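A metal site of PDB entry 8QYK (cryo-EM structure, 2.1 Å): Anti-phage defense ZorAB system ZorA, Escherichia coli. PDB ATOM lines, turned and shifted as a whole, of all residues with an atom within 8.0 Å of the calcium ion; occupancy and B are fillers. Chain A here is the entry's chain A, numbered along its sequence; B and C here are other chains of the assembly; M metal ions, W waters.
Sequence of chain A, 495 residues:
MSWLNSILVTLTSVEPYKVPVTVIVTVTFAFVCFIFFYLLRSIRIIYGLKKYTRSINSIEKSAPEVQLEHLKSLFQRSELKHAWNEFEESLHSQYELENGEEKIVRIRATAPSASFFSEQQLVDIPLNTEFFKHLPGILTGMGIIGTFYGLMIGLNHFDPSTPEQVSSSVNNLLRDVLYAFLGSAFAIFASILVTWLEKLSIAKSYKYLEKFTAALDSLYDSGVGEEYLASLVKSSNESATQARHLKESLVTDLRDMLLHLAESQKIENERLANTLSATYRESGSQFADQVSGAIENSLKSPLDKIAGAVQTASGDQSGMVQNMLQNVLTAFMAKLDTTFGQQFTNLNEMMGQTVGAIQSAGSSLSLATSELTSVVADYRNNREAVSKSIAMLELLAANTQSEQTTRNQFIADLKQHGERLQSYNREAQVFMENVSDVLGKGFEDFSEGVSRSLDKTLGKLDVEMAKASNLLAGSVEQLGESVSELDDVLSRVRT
The side-chain carboxylate of Asp 217 of chain B sits at hydrogen-bond distance from the backbone NH of Ser 113 of chain B (2.7 Å). The side-chain carboxylate (OD1) of Asp 221 of chain B lies close to the side-chain carboxylate (OE2) of Glu 89 (2.7 Å). The side-chain carboxylate (OE1) of Glu 89 lies close to the backbone NH (N) of Ser 222 of chain B, 3.4 Å away.
Of the 24 residues printed, 4 come within 4 Å of the calcium ion. Along chain A the residues within 4 Å of the calcium ion span positions 86 to 89.
The calcium ion is bound by O of Asp 217 of chain B (2.3 Å), water W2 (2.3 Å), O of Tyr 220 of chain B (2.3 Å), OE1 of Glu 89 (2.5 Å), OE1 of Glu 86 (2.6 Å), OE2 of Glu 89 (2.8 Å) and water W1 (2.8 Å). Slightly farther from the calcium ion lies OE2 of Glu 86 (3.1 Å).
Water W1 bridges the backbone carbonyl oxygen of Ser 218 of chain B and the side-chain carboxylate of Asp 221 of chain B.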
ATOM      1  N   HIS A  82     -14.274 -21.961 -22.331  1.00  0.00           N
ATOM      2  CA  HIS A  82     -15.232 -23.004 -22.659  1.00  0.00           C
ATOM      3  C   HIS A  82     -16.654 -22.460 -22.715  1.00  0.00           C
ATOM      4  O   HIS A  82     -17.436 -22.824 -23.606  1.00  0.00           O
ATOM      5  CB  HIS A  82     -15.133 -24.146 -21.655  1.00  0.00           C
ATOM      6  CG  HIS A  82     -16.237 -25.152 -21.770  1.00  0.00           C
ATOM      7  ND1 HIS A  82     -16.283 -26.082 -22.783  1.00  0.00           N
ATOM      8  CD2 HIS A  82     -17.340 -25.361 -21.019  1.00  0.00           C
ATOM      9  CE1 HIS A  82     -17.366 -26.826 -22.642  1.00  0.00           C
ATOM     10  NE2 HIS A  82     -18.027 -26.409 -21.581  1.00  0.00           N
ATOM     11  N   ASN A  85     -17.061 -20.634 -25.941  1.00  0.00           N
ATOM     12  CA  ASN A  85     -17.172 -21.534 -27.088  1.00  0.00           C
ATOM     13  C   ASN A  85     -18.573 -22.123 -27.181  1.00  0.00           C
ATOM     14  O   ASN A  85     -19.194 -22.139 -28.260  1.00  0.00           O
ATOM     15  CB  ASN A  85     -16.124 -22.636 -27.003  1.00  0.00           C
ATOM     16  CG  ASN A  85     -14.729 -22.146 -27.318  1.00  0.00           C
ATOM     17  OD1 ASN A  85     -14.553 -21.142 -27.992  1.00  0.00           O
ATOM     18  ND2 ASN A  85     -13.719 -22.858 -26.824  1.00  0.00           N
ATOM     19  N   GLU A  86     -19.112 -22.572 -26.048  1.00  0.00           N
ATOM     20  CA  GLU A  86     -20.460 -23.142 -26.049  1.00  0.00           C
ATOM     21  C   GLU A  86     -21.507 -22.084 -26.395  1.00  0.00           C
ATOM     22  O   GLU A  86     -22.432 -22.348 -27.179  1.00  0.00           O
ATOM     23  CB  GLU A  86     -20.747 -23.779 -24.690  1.00  0.00           C
ATOM     24  CG  GLU A  86     -19.802 -24.915 -24.344  1.00  0.00           C
ATOM     25  CD  GLU A  86     -19.758 -25.983 -25.413  1.00  0.00           C
ATOM     26  OE1 GLU A  86     -20.828 -26.431 -25.850  1.00  0.00           O
ATOM     27  OE2 GLU A  86     -18.643 -26.391 -25.815  1.00  0.00           O
ATOM     28  N   PHE A  87     -21.370 -20.894 -25.827  1.00  0.00           N
ATOM     29  CA  PHE A  87     -22.300 -19.806 -26.122  1.00  0.00           C
ATOM     30  C   PHE A  87     -22.254 -19.431 -27.590  1.00  0.00           C
ATOM     31  O   PHE A  87     -23.290 -19.151 -28.207  1.00  0.00           O
ATOM     32  CB  PHE A  87     -21.978 -18.594 -25.250  1.00  0.00           C
ATOM     33  CG  PHE A  87     -22.898 -17.428 -25.460  1.00  0.00           C
ATOM     34  CD1 PHE A  87     -24.257 -17.547 -25.202  1.00  0.00           C
ATOM     35  CD2 PHE A  87     -22.412 -16.222 -25.930  1.00  0.00           C
ATOM     36  CE1 PHE A  87     -25.098 -16.481 -25.398  1.00  0.00           C
ATOM     37  CE2 PHE A  87     -23.254 -15.157 -26.126  1.00  0.00           C
ATOM     38  CZ  PHE A  87     -24.598 -15.281 -25.860  1.00  0.00           C
ATOM     39  N   GLU A  89     -21.493 -21.427 -30.014  1.00  0.00           N
ATOM     40  CA  GLU A  89     -22.289 -22.459 -30.681  1.00  0.00           C
ATOM     41  C   GLU A  89     -23.777 -22.127 -30.603  1.00  0.00           C
ATOM     42  O   GLU A  89     -24.517 -22.362 -31.559  1.00  0.00           O
ATOM     43  CB  GLU A  89     -22.040 -23.828 -30.052  1.00  0.00           C
ATOM     44  CG  GLU A  89     -20.630 -24.335 -30.179  1.00  0.00           C
ATOM     45  CD  GLU A  89     -20.435 -25.636 -29.424  1.00  0.00           C
ATOM     46  OE1 GLU A  89     -21.422 -26.113 -28.827  1.00  0.00           O
ATOM     47  OE2 GLU A  89     -19.316 -26.166 -29.424  1.00  0.00           O
ATOM     48  N   SER A  90     -24.227 -21.596 -29.459  1.00  0.00           N
ATOM     49  CA  SER A  90     -25.655 -21.285 -29.327  1.00  0.00           C
ATOM     50  C   SER A  90     -26.066 -20.089 -30.175  1.00  0.00           C
ATOM     51  O   SER A  90     -27.250 -19.931 -30.468  1.00  0.00           O
ATOM     52  CB  SER A  90     -26.004 -21.045 -27.858  1.00  0.00           C
ATOM     53  OG  SER A  90     -25.526 -19.783 -27.408  1.00  0.00           O
ATOM     54  N   PHE A 116     -24.512 -20.777 -20.138  1.00  0.00           N
ATOM     55  CA  PHE A 116     -23.125 -21.175 -20.309  1.00  0.00           C
ATOM     56  C   PHE A 116     -22.192 -20.464 -19.350  1.00  0.00           C
ATOM     57  O   PHE A 116     -21.303 -21.089 -18.771  1.00  0.00           O
ATOM     58  CB  PHE A 116     -22.682 -20.919 -21.751  1.00  0.00           C
ATOM     59  CG  PHE A 116     -23.663 -21.426 -22.775  1.00  0.00           C
ATOM     60  CD1 PHE A 116     -23.669 -22.749 -23.153  1.00  0.00           C
ATOM     61  CD2 PHE A 116     -24.593 -20.571 -23.331  1.00  0.00           C
ATOM     62  CE1 PHE A 116     -24.572 -23.218 -24.081  1.00  0.00           C
ATOM     63  CE2 PHE A 116     -25.508 -21.034 -24.257  1.00  0.00           C
ATOM     64  CZ  PHE A 116     -25.492 -22.360 -24.637  1.00  0.00           C
ATOM     65  N   PHE B  87     -26.934 -39.888 -24.136  1.00  0.00           N
ATOM     66  CA  PHE B  87     -26.296 -38.727 -24.739  1.00  0.00           C
ATOM     67  C   PHE B  87     -26.071 -38.924 -26.222  1.00  0.00           C
ATOM     68  O   PHE B  87     -26.263 -38.002 -27.016  1.00  0.00           O
ATOM     69  CB  PHE B  87     -24.975 -38.435 -24.018  1.00  0.00           C
ATOM     70  CG  PHE B  87     -24.199 -37.312 -24.640  1.00  0.00           C
ATOM     71  CD1 PHE B  87     -24.670 -36.014 -24.592  1.00  0.00           C
ATOM     72  CD2 PHE B  87     -22.997 -37.554 -25.267  1.00  0.00           C
ATOM     73  CE1 PHE B  87     -23.949 -34.983 -25.159  1.00  0.00           C
ATOM     74  CE2 PHE B  87     -22.274 -36.533 -25.834  1.00  0.00           C
ATOM     75  CZ  PHE B  87     -22.752 -35.237 -25.776  1.00  0.00           C
ATOM     76  N   ARG B 108     -23.744 -33.306 -34.361  1.00  0.00           N
ATOM     77  CA  ARG B 108     -24.202 -32.105 -33.692  1.00  0.00           C
ATOM     78  C   ARG B 108     -24.774 -32.426 -32.317  1.00  0.00           C
ATOM     79  O   ARG B 108     -25.419 -33.466 -32.136  1.00  0.00           O
ATOM     80  CB  ARG B 108     -25.246 -31.376 -34.536  1.00  0.00           C
ATOM     81  CG  ARG B 108     -24.840 -31.238 -35.985  1.00  0.00           C
ATOM     82  CD  ARG B 108     -23.635 -30.336 -36.103  1.00  0.00           C
ATOM     83  NE  ARG B 108     -23.898 -28.996 -35.583  1.00  0.00           N
ATOM     84  CZ  ARG B 108     -24.323 -27.984 -36.317  1.00  0.00           C
ATOM     85  NH1 ARG B 108     -24.537 -28.117 -37.614  1.00  0.00           N
ATOM     86  NH2 ARG B 108     -24.534 -26.806 -35.745  1.00  0.00           N
ATOM     87  N   ALA B 109     -24.543 -31.540 -31.371  1.00  0.00           N
ATOM     88  CA  ALA B 109     -25.110 -31.670 -30.029  1.00  0.00           C
ATOM     89  C   ALA B 109     -26.473 -31.000 -29.989  1.00  0.00           C
ATOM     90  O   ALA B 109     -26.659 -29.905 -30.542  1.00  0.00           O
ATOM     91  CB  ALA B 109     -24.178 -31.043 -28.994  1.00  0.00           C
ATOM     92  N   ALA B 111     -28.260 -31.434 -26.789  1.00  0.00           N
ATOM     93  CA  ALA B 111     -28.386 -31.267 -25.350  1.00  0.00           C
ATOM     94  C   ALA B 111     -26.996 -31.142 -24.741  1.00  0.00           C
ATOM     95  O   ALA B 111     -26.023 -31.683 -25.296  1.00  0.00           O
ATOM     96  CB  ALA B 111     -29.127 -32.452 -24.710  1.00  0.00           C
ATOM     97  N   PRO B 112     -26.858 -30.434 -23.628  1.00  0.00           N
ATOM     98  CA  PRO B 112     -25.596 -30.469 -22.899  1.00  0.00           C
ATOM     99  C   PRO B 112     -25.349 -31.859 -22.318  1.00  0.00           C
ATOM    100  O   PRO B 112     -26.277 -32.570 -21.961  1.00  0.00           O
ATOM    101  CB  PRO B 112     -25.786 -29.428 -21.795  1.00  0.00           C
ATOM    102  CG  PRO B 112     -27.257 -29.321 -21.625  1.00  0.00           C
ATOM    103  CD  PRO B 112     -27.850 -29.562 -22.978  1.00  0.00           C
ATOM    104  N   SER B 113     -24.067 -32.228 -22.242  1.00  0.00           N
ATOM    105  CA  SER B 113     -23.724 -33.544 -21.711  1.00  0.00           C
ATOM    106  C   SER B 113     -24.093 -33.691 -20.246  1.00  0.00           C
ATOM    107  O   SER B 113     -24.328 -34.823 -19.789  1.00  0.00           O
ATOM    108  CB  SER B 113     -22.229 -33.812 -21.926  1.00  0.00           C
ATOM    109  OG  SER B 113     -21.443 -32.877 -21.201  1.00  0.00           O
ATOM    110  N   THR B 213     -17.842 -33.121 -18.186  1.00  0.00           N
ATOM    111  CA  THR B 213     -18.922 -32.721 -19.076  1.00  0.00           C
ATOM    112  C   THR B 213     -18.497 -31.623 -20.037  1.00  0.00           C
ATOM    113  O   THR B 213     -18.916 -31.614 -21.199  1.00  0.00           O
ATOM    114  CB  THR B 213     -20.159 -32.288 -18.281  1.00  0.00           C
ATOM    115  OG1 THR B 213     -19.810 -31.278 -17.341  1.00  0.00           O
ATOM    116  CG2 THR B 213     -20.789 -33.478 -17.567  1.00  0.00           C
ATOM    117  N   ALA B 214     -17.651 -30.691 -19.584  1.00  0.00           N
ATOM    118  CA  ALA B 214     -17.109 -29.680 -20.477  1.00  0.00           C
ATOM    119  C   ALA B 214     -16.273 -30.324 -21.582  1.00  0.00           C
ATOM    120  O   ALA B 214     -16.330 -29.897 -22.744  1.00  0.00           O
ATOM    121  CB  ALA B 214     -16.281 -28.657 -19.703  1.00  0.00           C
ATOM    122  N   ALA B 215     -15.485 -31.343 -21.239  1.00  0.00           N
ATOM    123  CA  ALA B 215     -14.755 -32.075 -22.262  1.00  0.00           C
ATOM    124  C   ALA B 215     -15.690 -32.713 -23.276  1.00  0.00           C
ATOM    125  O   ALA B 215     -15.468 -32.636 -24.490  1.00  0.00           O
ATOM    126  CB  ALA B 215     -13.857 -33.140 -21.619  1.00  0.00           C
ATOM    127  N   LEU B 216     -16.769 -33.359 -22.797  1.00  0.00           N
ATOM    128  CA  LEU B 216     -17.718 -33.970 -23.710  1.00  0.00           C
ATOM    129  C   LEU B 216     -18.413 -32.933 -24.595  1.00  0.00           C
ATOM    130  O   LEU B 216     -18.571 -33.152 -25.805  1.00  0.00           O
ATOM    131  CB  LEU B 216     -18.754 -34.778 -22.934  1.00  0.00           C
ATOM    132  CG  LEU B 216     -18.460 -36.272 -22.781  1.00  0.00           C
ATOM    133  CD1 LEU B 216     -19.622 -36.987 -22.113  1.00  0.00           C
ATOM    134  CD2 LEU B 216     -18.148 -36.914 -24.129  1.00  0.00           C
ATOM    135  N   ASP B 217     -18.811 -31.797 -24.013  1.00  0.00           N
ATOM    136  CA  ASP B 217     -19.530 -30.788 -24.781  1.00  0.00           C
ATOM    137  C   ASP B 217     -18.672 -30.190 -25.882  1.00  0.00           C
ATOM    138  O   ASP B 217     -19.183 -29.862 -26.957  1.00  0.00           O
ATOM    139  CB  ASP B 217     -20.036 -29.687 -23.845  1.00  0.00           C
ATOM    140  CG  ASP B 217     -21.297 -30.076 -23.121  1.00  0.00           C
ATOM    141  OD1 ASP B 217     -21.974 -31.024 -23.558  1.00  0.00           O
ATOM    142  OD2 ASP B 217     -21.624 -29.430 -22.094  1.00  0.00           O
ATOM    143  N   SER B 218     -17.368 -30.033 -25.647  1.00  0.00           N
ATOM    144  CA  SER B 218     -16.487 -29.405 -26.620  1.00  0.00           C
ATOM    145  C   SER B 218     -16.287 -30.242 -27.880  1.00  0.00           C
ATOM    146  O   SER B 218     -15.742 -29.727 -28.855  1.00  0.00           O
ATOM    147  CB  SER B 218     -15.138 -29.104 -25.965  1.00  0.00           C
ATOM    148  OG  SER B 218     -14.325 -30.254 -25.912  1.00  0.00           O
ATOM    149  N   LEU B 219     -16.706 -31.503 -27.872  1.00  0.00           N
ATOM    150  CA  LEU B 219     -16.557 -32.336 -29.053  1.00  0.00           C
ATOM    151  C   LEU B 219     -17.569 -31.987 -30.133  1.00  0.00           C
ATOM    152  O   LEU B 219     -17.255 -32.079 -31.332  1.00  0.00           O
ATOM    153  CB  LEU B 219     -16.711 -33.821 -28.689  1.00  0.00           C
ATOM    154  CG  LEU B 219     -15.650 -34.491 -27.820  1.00  0.00           C
ATOM    155  CD1 LEU B 219     -15.964 -35.958 -27.665  1.00  0.00           C
ATOM    156  CD2 LEU B 219     -14.263 -34.302 -28.390  1.00  0.00           C
ATOM    157  N   TYR B 220     -18.780 -31.591 -29.756  1.00  0.00           N
ATOM    158  CA  TYR B 220     -19.881 -31.441 -30.689  1.00  0.00           C
ATOM    159  C   TYR B 220     -20.521 -30.073 -30.559  1.00  0.00           C
ATOM    160  O   TYR B 220     -20.763 -29.577 -29.456  1.00  0.00           O
ATOM    161  CB  TYR B 220     -20.927 -32.542 -30.473  1.00  0.00           C
ATOM    162  CG  TYR B 220     -20.331 -33.924 -30.454  1.00  0.00           C
ATOM    163  CD1 TYR B 220     -19.845 -34.506 -31.610  1.00  0.00           C
ATOM    164  CD2 TYR B 220     -20.206 -34.634 -29.266  1.00  0.00           C
ATOM    165  CE1 TYR B 220     -19.292 -35.765 -31.601  1.00  0.00           C
ATOM    166  CE2 TYR B 220     -19.652 -35.892 -29.247  1.00  0.00           C
ATOM    167  CZ  TYR B 220     -19.197 -36.454 -30.420  1.00  0.00           C
ATOM    168  OH  TYR B 220     -18.635 -37.710 -30.413  1.00  0.00           O
ATOM    169  N   ASP B 221     -20.811 -29.461 -31.716  1.00  0.00           N
ATOM    170  CA  ASP B 221     -21.407 -28.142 -31.792  1.00  0.00           C
ATOM    171  C   ASP B 221     -22.928 -28.254 -31.783  1.00  0.00           C
ATOM    172  O   ASP B 221     -23.496 -29.188 -32.360  1.00  0.00           O
ATOM    173  CB  ASP B 221     -20.952 -27.417 -33.061  1.00  0.00           C
ATOM    174  CG  ASP B 221     -19.451 -27.185 -33.083  1.00  0.00           C
ATOM    175  OD1 ASP B 221     -18.903 -26.730 -32.070  1.00  0.00           O
ATOM    176  OD2 ASP B 221     -18.832 -27.469 -34.125  1.00  0.00           O
ATOM    177  N   SER B 222     -23.577 -27.297 -31.141  1.00  0.00           N
ATOM    178  CA  SER B 222     -25.025 -27.257 -31.031  1.00  0.00           C
ATOM    179  C   SER B 222     -25.605 -26.352 -32.119  1.00  0.00           C
ATOM    180  O   SER B 222     -24.901 -25.888 -33.016  1.00  0.00           O
ATOM    181  CB  SER B 222     -25.430 -26.794 -29.637  1.00  0.00           C
ATOM    182  OG  SER B 222     -25.303 -25.389 -29.516  1.00  0.00           O
ATOM    183  N   PHE C   6     -30.478 -26.063 -23.821  1.00  0.00           N
ATOM    184  CA  PHE C   6     -29.394 -25.366 -23.128  1.00  0.00           C
ATOM    185  C   PHE C   6     -29.967 -24.161 -22.380  1.00  0.00           C
ATOM    186  O   PHE C   6     -29.850 -23.006 -22.790  1.00  0.00           O
ATOM    187  CB  PHE C   6     -28.308 -24.943 -24.121  1.00  0.00           C
ATOM    188  CG  PHE C   6     -27.724 -26.070 -24.906  1.00  0.00           C
ATOM    189  CD1 PHE C   6     -28.390 -26.597 -25.998  1.00  0.00           C
ATOM    190  CD2 PHE C   6     -26.492 -26.602 -24.568  1.00  0.00           C
ATOM    191  CE1 PHE C   6     -27.849 -27.633 -26.731  1.00  0.00           C
ATOM    192  CE2 PHE C   6     -25.940 -27.634 -25.293  1.00  0.00           C
ATOM    193  CZ  PHE C   6     -26.627 -28.158 -26.382  1.00  0.00           C
HETATM  194 CA    CA M   1     -20.353 -28.088 -27.732  1.00  0.00          CA
HETATM  195  O   HOH W   1     -18.150 -28.085 -29.502  1.00  0.00           O
HETATM  196  O   HOH W   2     -22.386 -28.864 -26.966  1.00  0.00           O
